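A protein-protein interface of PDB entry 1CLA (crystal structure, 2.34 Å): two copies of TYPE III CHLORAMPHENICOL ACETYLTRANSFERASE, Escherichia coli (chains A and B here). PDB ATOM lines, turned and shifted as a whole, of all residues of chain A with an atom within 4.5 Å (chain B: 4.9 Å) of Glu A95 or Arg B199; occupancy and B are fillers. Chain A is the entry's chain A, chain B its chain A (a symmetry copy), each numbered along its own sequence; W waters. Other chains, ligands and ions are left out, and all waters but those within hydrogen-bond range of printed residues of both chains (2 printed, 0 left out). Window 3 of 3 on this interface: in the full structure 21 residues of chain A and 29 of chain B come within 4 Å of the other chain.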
ATOM      1  N   PHE A  90     -28.366 -15.613  -2.719  1.00  0.00           N
ATOM      2  CA  PHE A  90     -28.649 -16.070  -1.391  1.00  0.00           C
ATOM      3  C   PHE A  90     -28.738 -14.922  -0.405  1.00  0.00           C
ATOM      4  O   PHE A  90     -27.934 -14.001  -0.378  1.00  0.00           O
ATOM      5  CB  PHE A  90     -27.603 -17.100  -0.935  1.00  0.00           C
ATOM      6  CG  PHE A  90     -28.050 -17.830   0.299  1.00  0.00           C
ATOM      7  CD1 PHE A  90     -29.168 -18.658   0.320  1.00  0.00           C
ATOM      8  CD2 PHE A  90     -27.309 -17.701   1.465  1.00  0.00           C
ATOM      9  CE1 PHE A  90     -29.502 -19.354   1.475  1.00  0.00           C
ATOM     10  CE2 PHE A  90     -27.625 -18.384   2.626  1.00  0.00           C
ATOM     11  CZ  PHE A  90     -28.746 -19.223   2.624  1.00  0.00           C
ATOM     12  N   HIS A  91     -29.729 -14.966   0.480  1.00  0.00           N
ATOM     13  CA  HIS A  91     -29.909 -13.971   1.537  1.00  0.00           C
ATOM     14  C   HIS A  91     -29.574 -14.719   2.839  1.00  0.00           C
ATOM     15  O   HIS A  91     -30.354 -15.549   3.318  1.00  0.00           O
ATOM     16  CB  HIS A  91     -31.343 -13.458   1.598  1.00  0.00           C
ATOM     17  CG  HIS A  91     -31.776 -12.757   0.326  1.00  0.00           C
ATOM     18  ND1 HIS A  91     -31.154 -11.599  -0.130  1.00  0.00           N
ATOM     19  CD2 HIS A  91     -32.748 -13.052  -0.567  1.00  0.00           C
ATOM     20  CE1 HIS A  91     -31.745 -11.238  -1.255  1.00  0.00           C
ATOM     21  NE2 HIS A  91     -32.697 -12.096  -1.530  1.00  0.00           N
ATOM     22  N   GLN A  92     -28.407 -14.451   3.401  1.00  0.00           N
ATOM     23  CA  GLN A  92     -27.940 -15.192   4.597  1.00  0.00           C
ATOM     24  C   GLN A  92     -28.846 -14.971   5.827  1.00  0.00           C
ATOM     25  O   GLN A  92     -28.914 -15.820   6.727  1.00  0.00           O
ATOM     26  CB  GLN A  92     -26.507 -14.799   4.972  1.00  0.00           C
ATOM     27  CG  GLN A  92     -25.619 -16.025   5.234  1.00  0.00           C
ATOM     28  N   GLU A  93     -29.535 -13.844   5.856  1.00  0.00           N
ATOM     29  CA  GLU A  93     -30.413 -13.483   6.995  1.00  0.00           C
ATOM     30  C   GLU A  93     -31.714 -14.266   7.017  1.00  0.00           C
ATOM     31  O   GLU A  93     -32.227 -14.539   8.123  1.00  0.00           O
ATOM     32  CB  GLU A  93     -30.870 -12.020   6.924  1.00  0.00           C
ATOM     33  CG  GLU A  93     -29.733 -11.027   6.747  1.00  0.00           C
ATOM     34  CD  GLU A  93     -29.072 -11.143   5.382  1.00  0.00           C
ATOM     35  OE1 GLU A  93     -28.139 -10.319   5.050  1.00  0.00           O
ATOM     36  OE2 GLU A  93     -29.460 -12.060   4.568  1.00  0.00           O
ATOM     37  N   THR A  94     -32.302 -14.497   5.872  1.00  0.00           N
ATOM     38  CA  THR A  94     -33.587 -15.157   5.759  1.00  0.00           C
ATOM     39  C   THR A  94     -33.434 -16.600   5.382  1.00  0.00           C
ATOM     40  O   THR A  94     -34.349 -17.422   5.538  1.00  0.00           O
ATOM     41  CB  THR A  94     -34.519 -14.389   4.743  1.00  0.00           C
ATOM     42  OG1 THR A  94     -33.902 -14.429   3.409  1.00  0.00           O
ATOM     43  CG2 THR A  94     -34.823 -12.943   5.178  1.00  0.00           C
ATOM     44  N   GLU A  95     -32.282 -16.889   4.794  1.00  0.00           N
ATOM     45  CA  GLU A  95     -31.906 -18.235   4.269  1.00  0.00           C
ATOM     46  C   GLU A  95     -32.719 -18.651   3.040  1.00  0.00           C
ATOM     47  O   GLU A  95     -33.007 -19.802   2.773  1.00  0.00           O
ATOM     48  CB  GLU A  95     -31.954 -19.341   5.341  1.00  0.00           C
ATOM     49  CG  GLU A  95     -30.788 -19.275   6.334  1.00  0.00           C
ATOM     50  CD  GLU A  95     -30.814 -20.223   7.473  1.00  0.00           C
ATOM     51  OE1 GLU A  95     -31.697 -21.038   7.663  1.00  0.00           O
ATOM     52  OE2 GLU A  95     -29.780 -20.088   8.181  1.00  0.00           O
ATOM     53  N   THR A  96     -33.098 -17.640   2.243  1.00  0.00           N
ATOM     54  CA  THR A  96     -33.902 -17.758   1.054  1.00  0.00           C
ATOM     55  C   THR A  96     -33.106 -17.183  -0.105  1.00  0.00           C
ATOM     56  O   THR A  96     -32.155 -16.478   0.138  1.00  0.00           O
ATOM     57  CB  THR A  96     -35.290 -17.003   1.203  1.00  0.00           C
ATOM     58  OG1 THR A  96     -35.020 -15.588   1.421  1.00  0.00           O
ATOM     59  CG2 THR A  96     -36.206 -17.593   2.235  1.00  0.00           C
ATOM     60  N   PHE B  65     -34.131 -30.985  11.119  1.00  0.00           N
ATOM     61  CA  PHE B  65     -34.576 -29.938  10.189  1.00  0.00           C
ATOM     62  C   PHE B  65     -36.058 -30.084   9.801  1.00  0.00           C
ATOM     63  O   PHE B  65     -36.412 -31.120   9.235  1.00  0.00           O
ATOM     64  CB  PHE B  65     -33.686 -29.865   8.936  1.00  0.00           C
ATOM     65  CG  PHE B  65     -32.196 -29.809   9.214  1.00  0.00           C
ATOM     66  CD1 PHE B  65     -31.380 -30.912   8.989  1.00  0.00           C
ATOM     67  CD2 PHE B  65     -31.630 -28.687   9.764  1.00  0.00           C
ATOM     68  CE1 PHE B  65     -30.021 -30.871   9.249  1.00  0.00           C
ATOM     69  CE2 PHE B  65     -30.271 -28.626  10.063  1.00  0.00           C
ATOM     70  CZ  PHE B  65     -29.443 -29.731   9.803  1.00  0.00           C
ATOM     71  N   GLU B  67     -37.965 -28.521   7.413  1.00  0.00           N
ATOM     72  CA  GLU B  67     -38.201 -28.504   5.972  1.00  0.00           C
ATOM     73  C   GLU B  67     -38.137 -29.859   5.317  1.00  0.00           C
ATOM     74  O   GLU B  67     -38.824 -30.153   4.282  1.00  0.00           O
ATOM     75  CB  GLU B  67     -37.338 -27.454   5.253  1.00  0.00           C
ATOM     76  CG  GLU B  67     -35.864 -27.576   5.283  1.00  0.00           C
ATOM     77  CD  GLU B  67     -35.010 -27.251   6.462  1.00  0.00           C
ATOM     78  OE1 GLU B  67     -33.806 -27.522   6.430  1.00  0.00           O
ATOM     79  OE2 GLU B  67     -35.539 -26.645   7.434  1.00  0.00           O
ATOM     80  N   ASP B 193     -34.734 -25.883  -0.714  1.00  0.00           N
ATOM     81  CA  ASP B 193     -33.832 -25.140  -1.625  1.00  0.00           C
ATOM     82  C   ASP B 193     -32.512 -25.956  -1.620  1.00  0.00           C
ATOM     83  O   ASP B 193     -32.464 -26.976  -0.915  1.00  0.00           O
ATOM     84  CB  ASP B 193     -33.701 -23.683  -1.254  1.00  0.00           C
ATOM     85  CG  ASP B 193     -34.999 -22.914  -1.381  1.00  0.00           C
ATOM     86  OD1 ASP B 193     -35.109 -21.928  -0.626  1.00  0.00           O
ATOM     87  OD2 ASP B 193     -35.889 -23.267  -2.209  1.00  0.00           O
ATOM     88  N   PHE B 195     -29.748 -24.889  -0.592  1.00  0.00           N
ATOM     89  CA  PHE B 195     -29.197 -24.587   0.747  1.00  0.00           C
ATOM     90  C   PHE B 195     -29.606 -25.662   1.761  1.00  0.00           C
ATOM     91  O   PHE B 195     -28.772 -26.167   2.523  1.00  0.00           O
ATOM     92  CB  PHE B 195     -29.751 -23.265   1.306  1.00  0.00           C
ATOM     93  CG  PHE B 195     -29.288 -22.984   2.749  1.00  0.00           C
ATOM     94  CD1 PHE B 195     -30.159 -23.190   3.835  1.00  0.00           C
ATOM     95  CD2 PHE B 195     -27.988 -22.520   2.988  1.00  0.00           C
ATOM     96  CE1 PHE B 195     -29.726 -22.933   5.147  1.00  0.00           C
ATOM     97  CE2 PHE B 195     -27.556 -22.263   4.298  1.00  0.00           C
ATOM     98  CZ  PHE B 195     -28.426 -22.469   5.377  1.00  0.00           C
ATOM     99  N   HIS B 196     -30.897 -25.986   1.742  1.00  0.00           N
ATOM    100  CA  HIS B 196     -31.493 -26.950   2.694  1.00  0.00           C
ATOM    101  C   HIS B 196     -30.909 -28.341   2.514  1.00  0.00           C
ATOM    102  O   HIS B 196     -30.671 -29.048   3.526  1.00  0.00           O
ATOM    103  CB  HIS B 196     -33.011 -26.935   2.590  1.00  0.00           C
ATOM    104  CG  HIS B 196     -33.554 -25.556   2.960  1.00  0.00           C
ATOM    105  ND1 HIS B 196     -34.082 -24.704   2.002  1.00  0.00           N
ATOM    106  CD2 HIS B 196     -33.630 -24.891   4.146  1.00  0.00           C
ATOM    107  CE1 HIS B 196     -34.442 -23.585   2.599  1.00  0.00           C
ATOM    108  NE2 HIS B 196     -34.178 -23.678   3.878  1.00  0.00           N
ATOM    109  N   VAL B 197     -30.608 -28.727   1.277  1.00  0.00           N
ATOM    110  CA  VAL B 197     -30.002 -29.989   0.887  1.00  0.00           C
ATOM    111  C   VAL B 197     -28.526 -30.007   1.292  1.00  0.00           C
ATOM    112  O   VAL B 197     -28.080 -30.999   1.884  1.00  0.00           O
ATOM    113  CB  VAL B 197     -30.268 -30.381  -0.576  1.00  0.00           C
ATOM    114  CG1 VAL B 197     -29.507 -31.708  -0.896  1.00  0.00           C
ATOM    115  CG2 VAL B 197     -31.741 -30.657  -0.831  1.00  0.00           C
ATOM    116  N   ALA B 198     -27.781 -28.914   1.045  1.00  0.00           N
ATOM    117  CA  ALA B 198     -26.387 -28.794   1.391  1.00  0.00           C
ATOM    118  C   ALA B 198     -26.263 -28.945   2.905  1.00  0.00           C
ATOM    119  O   ALA B 198     -25.423 -29.734   3.415  1.00  0.00           O
ATOM    120  CB  ALA B 198     -25.616 -27.566   0.845  1.00  0.00           C
ATOM    121  N   ARG B 199     -27.091 -28.265   3.674  1.00  0.00           N
ATOM    122  CA  ARG B 199     -27.162 -28.259   5.128  1.00  0.00           C
ATOM    123  C   ARG B 199     -27.298 -29.662   5.728  1.00  0.00           C
ATOM    124  O   ARG B 199     -26.590 -30.036   6.694  1.00  0.00           O
ATOM    125  CB  ARG B 199     -28.244 -27.294   5.681  1.00  0.00           C
ATOM    126  CG  ARG B 199     -28.209 -27.147   7.162  1.00  0.00           C
ATOM    127  CD  ARG B 199     -28.944 -26.050   7.838  1.00  0.00           C
ATOM    128  NE  ARG B 199     -30.370 -26.169   7.677  1.00  0.00           N
ATOM    129  CZ  ARG B 199     -31.302 -25.225   7.854  1.00  0.00           C
ATOM    130  NH1 ARG B 199     -30.937 -24.010   8.272  1.00  0.00           N
ATOM    131  NH2 ARG B 199     -32.613 -25.495   7.608  1.00  0.00           N
ATOM    132  N   PHE B 200     -28.161 -30.466   5.202  1.00  0.00           N
ATOM    133  CA  PHE B 200     -28.475 -31.824   5.533  1.00  0.00           C
ATOM    134  C   PHE B 200     -27.228 -32.686   5.297  1.00  0.00           C
ATOM    135  O   PHE B 200     -26.990 -33.534   6.097  1.00  0.00           O
ATOM    136  CB  PHE B 200     -29.624 -32.471   4.687  1.00  0.00           C
ATOM    137  CG  PHE B 200     -29.724 -33.935   4.734  1.00  0.00           C
ATOM    138  CD1 PHE B 200     -30.082 -34.604   5.909  1.00  0.00           C
ATOM    139  CD2 PHE B 200     -29.358 -34.687   3.598  1.00  0.00           C
ATOM    140  CE1 PHE B 200     -30.131 -35.995   5.955  1.00  0.00           C
ATOM    141  CE2 PHE B 200     -29.371 -36.089   3.660  1.00  0.00           C
ATOM    142  CZ  PHE B 200     -29.737 -36.753   4.853  1.00  0.00           C
ATOM    143  N   ILE B 201     -26.644 -32.546   4.146  1.00  0.00           N
ATOM    144  CA  ILE B 201     -25.459 -33.329   3.764  1.00  0.00           C
ATOM    145  C   ILE B 201     -24.294 -32.987   4.694  1.00  0.00           C
ATOM    146  O   ILE B 201     -23.605 -33.859   5.300  1.00  0.00           O
ATOM    147  CB  ILE B 201     -25.218 -33.149   2.243  1.00  0.00           C
ATOM    148  CG1 ILE B 201     -26.317 -33.968   1.474  1.00  0.00           C
ATOM    149  CG2 ILE B 201     -23.796 -33.503   1.786  1.00  0.00           C
ATOM    150  CD1 ILE B 201     -26.634 -33.433   0.077  1.00  0.00           C
ATOM    151  N   ASN B 202     -24.054 -31.698   4.917  1.00  0.00           N
ATOM    152  CA  ASN B 202     -22.998 -31.183   5.783  1.00  0.00           C
ATOM    153  C   ASN B 202     -23.230 -31.706   7.195  1.00  0.00           C
ATOM    154  O   ASN B 202     -22.256 -32.219   7.792  1.00  0.00           O
ATOM    155  CB  ASN B 202     -22.904 -29.675   5.646  1.00  0.00           C
ATOM    156  CG  ASN B 202     -22.340 -29.236   4.310  1.00  0.00           C
ATOM    157  OD1 ASN B 202     -21.690 -30.018   3.587  1.00  0.00           O
ATOM    158  ND2 ASN B 202     -22.626 -27.991   3.992  1.00  0.00           N
ATOM    159  N   ARG B 203     -24.453 -31.622   7.683  1.00  0.00           N
ATOM    160  CA  ARG B 203     -24.874 -32.173   8.956  1.00  0.00           C
ATOM    161  C   ARG B 203     -24.664 -33.689   8.989  1.00  0.00           C
ATOM    162  O   ARG B 203     -24.206 -34.183  10.033  1.00  0.00           O
ATOM    163  CB  ARG B 203     -26.311 -31.864   9.374  1.00  0.00           C
ATOM    164  CG  ARG B 203     -26.749 -32.480  10.715  1.00  0.00           C
ATOM    165  CD  ARG B 203     -25.889 -32.016  11.814  1.00  0.00           C
ATOM    166  NE  ARG B 203     -26.269 -32.401  13.105  1.00  0.00           N
ATOM    167  CZ  ARG B 203     -25.508 -32.660  14.162  1.00  0.00           C
ATOM    168  NH1 ARG B 203     -24.177 -32.589  14.152  1.00  0.00           N
ATOM    169  NH2 ARG B 203     -26.131 -33.044  15.284  1.00  0.00           N
ATOM    170  N   LEU B 204     -25.034 -34.434   7.960  1.00  0.00           N
ATOM    171  CA  LEU B 204     -24.814 -35.876   7.846  1.00  0.00           C
ATOM    172  C   LEU B 204     -23.337 -36.277   7.891  1.00  0.00           C
ATOM    173  O   LEU B 204     -22.909 -37.155   8.652  1.00  0.00           O
ATOM    174  CB  LEU B 204     -25.500 -36.404   6.583  1.00  0.00           C
ATOM    175  CG  LEU B 204     -25.276 -37.899   6.332  1.00  0.00           C
ATOM    176  CD1 LEU B 204     -25.831 -38.714   7.515  1.00  0.00           C
ATOM    177  CD2 LEU B 204     -26.071 -38.224   5.063  1.00  0.00           C
HETATM  178  O   HOH W   1     -35.471 -20.644   4.818  1.00  0.00           O
HETATM  179  O   HOH W   2     -32.788 -20.984   0.454  1.00  0.00           O
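The side-chain carboxylate of Glu A95 is in salt-bridge range of the guanidinium group of Arg B199 (3.1 Å).
Glu A95 touches just these residues of chain B: Phe B195 and Arg B199. Of chain A, only Glu A95 (3.1 Å) comes within 4 Å of Arg B199. Of the printed residues of chain B, Phe A90 touches Phe B195 (3.4 Å). Of the printed residues of chain A, Phe B195 touches Phe A90 (3.4 Å) and Glu A95 (3.7 Å). The nearest printed residue of chain A that does not touch Arg B199 is Phe A90 (7.7 Å). The nearest printed residue of chain B that does not touch Phe A90 is Asp B193 (6.5 Å).
Among the printed residues, pairs that only touch across the chains: Phe A90 with Phe B195 and Glu A95 with Phe B195.
No position is printed for both chains. Of the 3 pairs that touch across the chains among the printed residues, none has its exchanged pair printed and touching as well.
Hydrophobic or aromatic side chains of chain A within 4 Å of the printed part of chain B: Phe A90. Of the 13 printed residues of chain B, 2 touch a printed residue of chain A. Hydrophobic or aromatic side chains of chain B that line the printed part of chain A: Phe B195. Among the printed residues, 3 pairs touch across the chains. Among the printed residues, Asp or Glu carboxylates within 4 Å of a Lys or Arg side-chain nitrogen of the other chain: Glu A95 with Arg B199 (3.1 Å).
The guanidinium group of Arg B199 lies within salt-bridge range of the side-chain carboxylate of Glu B67 (2.6 Å).
Water W2 lies within hydrogen-bond range of O of Glu A95 and OD1 of Asp B193. Water W1 lies within hydrogen-bond range of O of Glu A95 (3.3 Å), NE2 of His B196 (3.4 Å) and O of Thr A94 (3.5 Å).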
